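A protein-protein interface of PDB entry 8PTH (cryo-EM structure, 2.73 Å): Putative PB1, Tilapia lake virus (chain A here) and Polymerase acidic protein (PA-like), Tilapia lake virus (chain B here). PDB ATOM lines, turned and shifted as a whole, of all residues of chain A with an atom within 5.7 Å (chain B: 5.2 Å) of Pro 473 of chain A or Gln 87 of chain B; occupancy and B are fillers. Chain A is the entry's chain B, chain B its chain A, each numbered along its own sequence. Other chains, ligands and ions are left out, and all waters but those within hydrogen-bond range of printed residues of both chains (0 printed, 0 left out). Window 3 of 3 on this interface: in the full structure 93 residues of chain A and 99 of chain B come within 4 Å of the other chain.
Leu 471 of chain A touches Gln 87 of chain B.
Val 472 of chain A touches Gln 84 of chain B (CG1 to NE2, 3.4 Å).
Tyr 79 of chain B touches Pro 473 of chain A.
Pro 473 of chain A touches Val 80 of chain B.
CG of Pro 473 of chain A touches NE2 of Gln 87 of chain B, at 3.1 Å.
Val 80 of chain B touches Leu 476 of chain A.
CD1 of Leu 476 of chain A touches C of Cys 81 of chain B, 3.6 Å away.
O of Glu 83 of chain B lies close to SG of Cys 81 of chain B (3.8 Å).
The side-chain sulfur of Cys 71 of chain B sits close to the backbone carbonyl oxygen of Val 80 of chain B (3.6 Å).
OE1 of Gln 84 of chain B sits close to OE1 of Gln 87 of chain B, 2.6 Å away.
O of Tyr 79 of chain B sits at hydrogen-bond distance from NE2 of Gln 87 of chain B (3.0 Å).
O of Gln 87 of chain B sits at hydrogen-bond distance from SG of Cys 90 of chain B.
Of the 7 printed residues of chain A, 4 touch a printed residue of chain B.
Hydrophobic or aromatic side chains of chain A that line the printed part of chain B: Leu 471, Val 472, Pro 473 and Leu 476.
Of the 14 printed residues of chain B, 5 touch a printed residue of chain A.
Hydrophobic or aromatic side chains of chain B that line the printed part of chain A: Val 80.
Among the printed residues, no Asp or Glu carboxylate lies within 4 Å of a Lys or Arg side-chain nitrogen of the other chain.
The side-chain amide oxygen of Gln 84 of chain B lies close to the backbone carbonyl oxygen of Leu 471 of chain A (2.7 Å).
Printed residues of chain B within 4 Å of Val 472 of chain A: Gln 84 (3.4 Å).
Of chain B, only Tyr 79, Val 80 and Gln 87 come within 4 Å of Pro 473 of chain A.
Printed residues of chain B within 4 Å of Leu 476 of chain A: Val 80 (3.6 Å) and Cys 81 (3.6 Å).
Printed residues of chain A within 4 Å of Tyr 79 of chain B: Pro 473 (3.8 Å).
Of the printed residues of chain A, Val 80 of chain B touches Pro 473 (3.8 Å) and Leu 476 (3.6 Å).
Printed residues of chain A within 4 Å of Gln 84 of chain B: Leu 471 and Val 472.
Glu 85 of chain B touches none of the printed residues of chain A.
Gln 87 of chain B touches just these residues of chain A: Leu 471 (3.5 Å) and Pro 473 (3.1 Å).
The nearest residue of chain A that does not touch Gln 87 of chain B is Val 472 of chain A (4.8 Å).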
ATOM      1  N   PRO A 470     -17.612  27.818 -17.582  1.00  0.00           N
ATOM      2  CA  PRO A 470     -18.551  27.553 -16.478  1.00  0.00           C
ATOM      3  C   PRO A 470     -18.071  26.492 -15.504  1.00  0.00           C
ATOM      4  O   PRO A 470     -18.632  26.387 -14.406  1.00  0.00           O
ATOM      5  CB  PRO A 470     -19.828  27.106 -17.201  1.00  0.00           C
ATOM      6  CG  PRO A 470     -19.732  27.688 -18.555  1.00  0.00           C
ATOM      7  CD  PRO A 470     -18.276  27.744 -18.897  1.00  0.00           C
ATOM      8  N   LEU A 471     -17.062  25.701 -15.862  1.00  0.00           N
ATOM      9  CA  LEU A 471     -16.609  24.603 -15.019  1.00  0.00           C
ATOM     10  C   LEU A 471     -15.516  25.000 -14.034  1.00  0.00           C
ATOM     11  O   LEU A 471     -15.146  24.179 -13.189  1.00  0.00           O
ATOM     12  CB  LEU A 471     -16.103  23.445 -15.891  1.00  0.00           C
ATOM     13  CG  LEU A 471     -17.158  22.591 -16.602  1.00  0.00           C
ATOM     14  CD1 LEU A 471     -17.734  21.563 -15.644  1.00  0.00           C
ATOM     15  CD2 LEU A 471     -18.272  23.441 -17.199  1.00  0.00           C
ATOM     16  N   VAL A 472     -14.992  26.219 -14.110  1.00  0.00           N
ATOM     17  CA  VAL A 472     -13.960  26.686 -13.189  1.00  0.00           C
ATOM     18  C   VAL A 472     -14.657  27.305 -11.979  1.00  0.00           C
ATOM     19  O   VAL A 472     -15.490  28.208 -12.157  1.00  0.00           O
ATOM     20  CB  VAL A 472     -13.007  27.690 -13.852  1.00  0.00           C
ATOM     21  CG1 VAL A 472     -12.516  27.165 -15.196  1.00  0.00           C
ATOM     22  CG2 VAL A 472     -13.668  29.054 -14.014  1.00  0.00           C
ATOM     23  N   PRO A 473     -14.382  26.845 -10.761  1.00  0.00           N
ATOM     24  CA  PRO A 473     -14.960  27.504  -9.587  1.00  0.00           C
ATOM     25  C   PRO A 473     -14.402  28.904  -9.403  1.00  0.00           C
ATOM     26  O   PRO A 473     -13.285  29.214  -9.821  1.00  0.00           O
ATOM     27  CB  PRO A 473     -14.558  26.591  -8.423  1.00  0.00           C
ATOM     28  CG  PRO A 473     -14.162  25.305  -9.048  1.00  0.00           C
ATOM     29  CD  PRO A 473     -13.606  25.652 -10.384  1.00  0.00           C
ATOM     30  N   HIS A 474     -15.201  29.754  -8.763  1.00  0.00           N
ATOM     31  CA  HIS A 474     -14.765  31.108  -8.461  1.00  0.00           C
ATOM     32  C   HIS A 474     -13.841  31.173  -7.254  1.00  0.00           C
ATOM     33  O   HIS A 474     -13.315  32.249  -6.954  1.00  0.00           O
ATOM     34  CB  HIS A 474     -15.978  32.011  -8.231  1.00  0.00           C
ATOM     35  CG  HIS A 474     -16.631  32.479  -9.494  1.00  0.00           C
ATOM     36  ND1 HIS A 474     -16.207  32.084 -10.745  1.00  0.00           N
ATOM     37  CD2 HIS A 474     -17.676  33.316  -9.700  1.00  0.00           C
ATOM     38  CE1 HIS A 474     -16.963  32.653 -11.665  1.00  0.00           C
ATOM     39  NE2 HIS A 474     -17.862  33.407 -11.058  1.00  0.00           N
ATOM     40  N   ARG A 475     -13.632  30.058  -6.557  1.00  0.00           N
ATOM     41  CA  ARG A 475     -12.705  29.998  -5.436  1.00  0.00           C
ATOM     42  C   ARG A 475     -11.297  29.598  -5.856  1.00  0.00           C
ATOM     43  O   ARG A 475     -10.415  29.501  -4.997  1.00  0.00           O
ATOM     44  CB  ARG A 475     -13.222  29.014  -4.381  1.00  0.00           C
ATOM     45  CG  ARG A 475     -14.316  29.584  -3.493  1.00  0.00           C
ATOM     46  CD  ARG A 475     -14.570  28.709  -2.276  1.00  0.00           C
ATOM     47  NE  ARG A 475     -14.785  29.501  -1.071  1.00  0.00           N
ATOM     48  CZ  ARG A 475     -15.016  28.993   0.133  1.00  0.00           C
ATOM     49  NH1 ARG A 475     -15.069  27.687   0.334  1.00  0.00           N
ATOM     50  NH2 ARG A 475     -15.199  29.816   1.160  1.00  0.00           N
ATOM     51  N   LEU A 476     -11.065  29.364  -7.144  1.00  0.00           N
ATOM     52  CA  LEU A 476      -9.734  29.008  -7.614  1.00  0.00           C
ATOM     53  C   LEU A 476      -8.791  30.197  -7.487  1.00  0.00           C
ATOM     54  O   LEU A 476      -9.157  31.337  -7.786  1.00  0.00           O
ATOM     55  CB  LEU A 476      -9.800  28.535  -9.066  1.00  0.00           C
ATOM     56  CG  LEU A 476      -8.476  28.157  -9.734  1.00  0.00           C
ATOM     57  CD1 LEU A 476      -8.091  26.731  -9.387  1.00  0.00           C
ATOM     58  CD2 LEU A 476      -8.575  28.338 -11.239  1.00  0.00           C
ATOM     59  N   CYS B  71      -5.281  20.260  -5.178  1.00  0.00           N
ATOM     60  CA  CYS B  71      -6.713  20.026  -5.338  1.00  0.00           C
ATOM     61  C   CYS B  71      -7.388  20.308  -4.002  1.00  0.00           C
ATOM     62  O   CYS B  71      -7.206  19.558  -3.036  1.00  0.00           O
ATOM     63  CB  CYS B  71      -6.982  18.597  -5.805  1.00  0.00           C
ATOM     64  SG  CYS B  71      -8.583  18.369  -6.610  1.00  0.00           S
ATOM     65  N   TYR B  79     -15.187  20.829  -4.951  1.00  0.00           N
ATOM     66  CA  TYR B  79     -13.752  20.697  -5.140  1.00  0.00           C
ATOM     67  C   TYR B  79     -13.261  21.684  -6.190  1.00  0.00           C
ATOM     68  O   TYR B  79     -13.994  22.064  -7.107  1.00  0.00           O
ATOM     69  CB  TYR B  79     -13.386  19.274  -5.557  1.00  0.00           C
ATOM     70  CG  TYR B  79     -14.139  18.207  -4.798  1.00  0.00           C
ATOM     71  CD1 TYR B  79     -13.672  17.734  -3.581  1.00  0.00           C
ATOM     72  CD2 TYR B  79     -15.317  17.673  -5.298  1.00  0.00           C
ATOM     73  CE1 TYR B  79     -14.356  16.758  -2.884  1.00  0.00           C
ATOM     74  CE2 TYR B  79     -16.010  16.698  -4.609  1.00  0.00           C
ATOM     75  CZ  TYR B  79     -15.524  16.244  -3.402  1.00  0.00           C
ATOM     76  OH  TYR B  79     -16.209  15.272  -2.710  1.00  0.00           O
ATOM     77  N   VAL B  80     -12.005  22.096  -6.040  1.00  0.00           N
ATOM     78  CA  VAL B  80     -11.379  23.070  -6.922  1.00  0.00           C
ATOM     79  C   VAL B  80     -10.012  22.545  -7.337  1.00  0.00           C
ATOM     80  O   VAL B  80      -9.303  21.917  -6.546  1.00  0.00           O
ATOM     81  CB  VAL B  80     -11.245  24.452  -6.245  1.00  0.00           C
ATOM     82  CG1 VAL B  80     -10.774  25.493  -7.245  1.00  0.00           C
ATOM     83  CG2 VAL B  80     -12.564  24.862  -5.607  1.00  0.00           C
ATOM     84  N   CYS B  81      -9.646  22.800  -8.590  1.00  0.00           N
ATOM     85  CA  CYS B  81      -8.332  22.410  -9.082  1.00  0.00           C
ATOM     86  C   CYS B  81      -7.964  23.288 -10.268  1.00  0.00           C
ATOM     87  O   CYS B  81      -8.811  23.580 -11.116  1.00  0.00           O
ATOM     88  CB  CYS B  81      -8.300  20.932  -9.485  1.00  0.00           C
ATOM     89  SG  CYS B  81      -6.645  20.210  -9.505  1.00  0.00           S
ATOM     90  N   GLU B  83      -6.319  22.434 -12.726  1.00  0.00           N
ATOM     91  CA  GLU B  83      -6.526  21.603 -13.903  1.00  0.00           C
ATOM     92  C   GLU B  83      -7.942  21.042 -13.854  1.00  0.00           C
ATOM     93  O   GLU B  83      -8.306  20.346 -12.900  1.00  0.00           O
ATOM     94  CB  GLU B  83      -5.498  20.473 -13.957  1.00  0.00           C
ATOM     95  CG  GLU B  83      -4.380  20.698 -14.963  1.00  0.00           C
ATOM     96  CD  GLU B  83      -3.554  21.934 -14.652  1.00  0.00           C
ATOM     97  OE1 GLU B  83      -2.712  21.872 -13.731  1.00  0.00           O
ATOM     98  OE2 GLU B  83      -3.747  22.967 -15.326  1.00  0.00           O
ATOM     99  N   GLN B  84      -8.735  21.344 -14.886  1.00  0.00           N
ATOM    100  CA  GLN B  84     -10.126  20.906 -14.904  1.00  0.00           C
ATOM    101  C   GLN B  84     -10.232  19.389 -14.813  1.00  0.00           C
ATOM    102  O   GLN B  84     -11.146  18.859 -14.171  1.00  0.00           O
ATOM    103  CB  GLN B  84     -10.815  21.409 -16.173  1.00  0.00           C
ATOM    104  CG  GLN B  84     -12.329  21.476 -16.077  1.00  0.00           C
ATOM    105  CD  GLN B  84     -12.812  22.673 -15.286  1.00  0.00           C
ATOM    106  OE1 GLN B  84     -13.230  22.544 -14.137  1.00  0.00           O
ATOM    107  NE2 GLN B  84     -12.763  23.846 -15.903  1.00  0.00           N
ATOM    108  N   GLU B  85      -9.308  18.676 -15.458  1.00  0.00           N
ATOM    109  CA  GLU B  85      -9.402  17.221 -15.499  1.00  0.00           C
ATOM    110  C   GLU B  85      -9.373  16.632 -14.096  1.00  0.00           C
ATOM    111  O   GLU B  85     -10.278  15.882 -13.710  1.00  0.00           O
ATOM    112  CB  GLU B  85      -8.264  16.653 -16.346  1.00  0.00           C
ATOM    113  CG  GLU B  85      -8.308  15.145 -16.506  1.00  0.00           C
ATOM    114  CD  GLU B  85      -7.174  14.623 -17.356  1.00  0.00           C
ATOM    115  OE1 GLU B  85      -6.308  15.429 -17.754  1.00  0.00           O
ATOM    116  OE2 GLU B  85      -7.147  13.406 -17.631  1.00  0.00           O
ATOM    117  N   TYR B  86      -8.353  16.983 -13.308  1.00  0.00           N
ATOM    118  CA  TYR B  86      -8.239  16.437 -11.961  1.00  0.00           C
ATOM    119  C   TYR B  86      -9.425  16.856 -11.105  1.00  0.00           C
ATOM    120  O   TYR B  86      -9.883  16.090 -10.248  1.00  0.00           O
ATOM    121  CB  TYR B  86      -6.927  16.884 -11.315  1.00  0.00           C
ATOM    122  CG  TYR B  86      -5.688  16.542 -12.113  1.00  0.00           C
ATOM    123  CD1 TYR B  86      -5.530  15.290 -12.693  1.00  0.00           C
ATOM    124  CD2 TYR B  86      -4.673  17.474 -12.285  1.00  0.00           C
ATOM    125  CE1 TYR B  86      -4.396  14.977 -13.421  1.00  0.00           C
ATOM    126  CE2 TYR B  86      -3.539  17.172 -13.010  1.00  0.00           C
ATOM    127  CZ  TYR B  86      -3.404  15.923 -13.576  1.00  0.00           C
ATOM    128  OH  TYR B  86      -2.274  15.623 -14.300  1.00  0.00           O
ATOM    129  N   GLN B  87      -9.936  18.069 -11.322  1.00  0.00           N
ATOM    130  CA  GLN B  87     -11.146  18.488 -10.626  1.00  0.00           C
ATOM    131  C   GLN B  87     -12.292  17.528 -10.910  1.00  0.00           C
ATOM    132  O   GLN B  87     -13.003  17.107  -9.994  1.00  0.00           O
ATOM    133  CB  GLN B  87     -11.539  19.906 -11.039  1.00  0.00           C
ATOM    134  CG  GLN B  87     -12.757  20.420 -10.294  1.00  0.00           C
ATOM    135  CD  GLN B  87     -13.144  21.823 -10.700  1.00  0.00           C
ATOM    136  OE1 GLN B  87     -12.534  22.421 -11.585  1.00  0.00           O
ATOM    137  NE2 GLN B  87     -14.184  22.349 -10.068  1.00  0.00           N
ATOM    138  N   GLN B  88     -12.492  17.178 -12.182  1.00  0.00           N
ATOM    139  CA  GLN B  88     -13.586  16.274 -12.525  1.00  0.00           C
ATOM    140  C   GLN B  88     -13.369  14.890 -11.923  1.00  0.00           C
ATOM    141  O   GLN B  88     -14.307  14.279 -11.390  1.00  0.00           O
ATOM    142  CB  GLN B  88     -13.733  16.187 -14.043  1.00  0.00           C
ATOM    143  CG  GLN B  88     -14.634  17.260 -14.633  1.00  0.00           C
ATOM    144  CD  GLN B  88     -16.105  16.935 -14.477  1.00  0.00           C
ATOM    145  OE1 GLN B  88     -16.504  16.256 -13.530  1.00  0.00           O
ATOM    146  NE2 GLN B  88     -16.921  17.420 -15.405  1.00  0.00           N
ATOM    147  N   ILE B  89     -12.137  14.378 -11.995  1.00  0.00           N
ATOM    148  CA  ILE B  89     -11.858  13.062 -11.418  1.00  0.00           C
ATOM    149  C   ILE B  89     -12.181  13.062  -9.932  1.00  0.00           C
ATOM    150  O   ILE B  89     -12.864  12.164  -9.427  1.00  0.00           O
ATOM    151  CB  ILE B  89     -10.399  12.632 -11.668  1.00  0.00           C
ATOM    152  CG1 ILE B  89      -9.949  12.943 -13.095  1.00  0.00           C
ATOM    153  CG2 ILE B  89     -10.235  11.155 -11.395  1.00  0.00           C
ATOM    154  CD1 ILE B  89      -8.570  12.417 -13.426  1.00  0.00           C
ATOM    155  N   CYS B  90     -11.695  14.070  -9.208  1.00  0.00           N
ATOM    156  CA  CYS B  90     -11.954  14.131  -7.776  1.00  0.00           C
ATOM    157  C   CYS B  90     -13.441  14.306  -7.490  1.00  0.00           C
ATOM    158  O   CYS B  90     -13.971  13.706  -6.549  1.00  0.00           O
ATOM    159  CB  CYS B  90     -11.143  15.265  -7.154  1.00  0.00           C
ATOM    160  SG  CYS B  90     -12.035  16.817  -7.042  1.00  0.00           S
ATOM    161  N   LYS B  91     -14.131  15.116  -8.294  1.00  0.00           N
ATOM    162  CA  LYS B  91     -15.554  15.350  -8.074  1.00  0.00           C
ATOM    163  C   LYS B  91     -16.343  14.055  -8.184  1.00  0.00           C
ATOM    164  O   LYS B  91     -17.192  13.757  -7.336  1.00  0.00           O
ATOM    165  CB  LYS B  91     -16.069  16.385  -9.076  1.00  0.00           C
ATOM    166  CG  LYS B  91     -17.558  16.287  -9.373  1.00  0.00           C
ATOM    167  CD  LYS B  91     -18.076  17.541 -10.061  1.00  0.00           C
ATOM    168  CE  LYS B  91     -19.562  17.736  -9.811  1.00  0.00           C
ATOM    169  NZ  LYS B  91     -20.161  18.728 -10.746  1.00  0.00           N
ATOM    170  N   VAL B  92     -16.079  13.267  -9.226  1.00  0.00           N
ATOM    171  CA  VAL B  92     -16.798  12.004  -9.373  1.00  0.00           C
ATOM    172  C   VAL B  92     -16.355  11.002  -8.313  1.00  0.00           C
ATOM    173  O   VAL B  92     -17.168  10.220  -7.806  1.00  0.00           O
ATOM    174  CB  VAL B  92     -16.641  11.443 -10.800  1.00  0.00           C
ATOM    175  CG1 VAL B  92     -16.946  12.517 -11.838  1.00  0.00           C
ATOM    176  CG2 VAL B  92     -15.243  10.882 -11.017  1.00  0.00           C
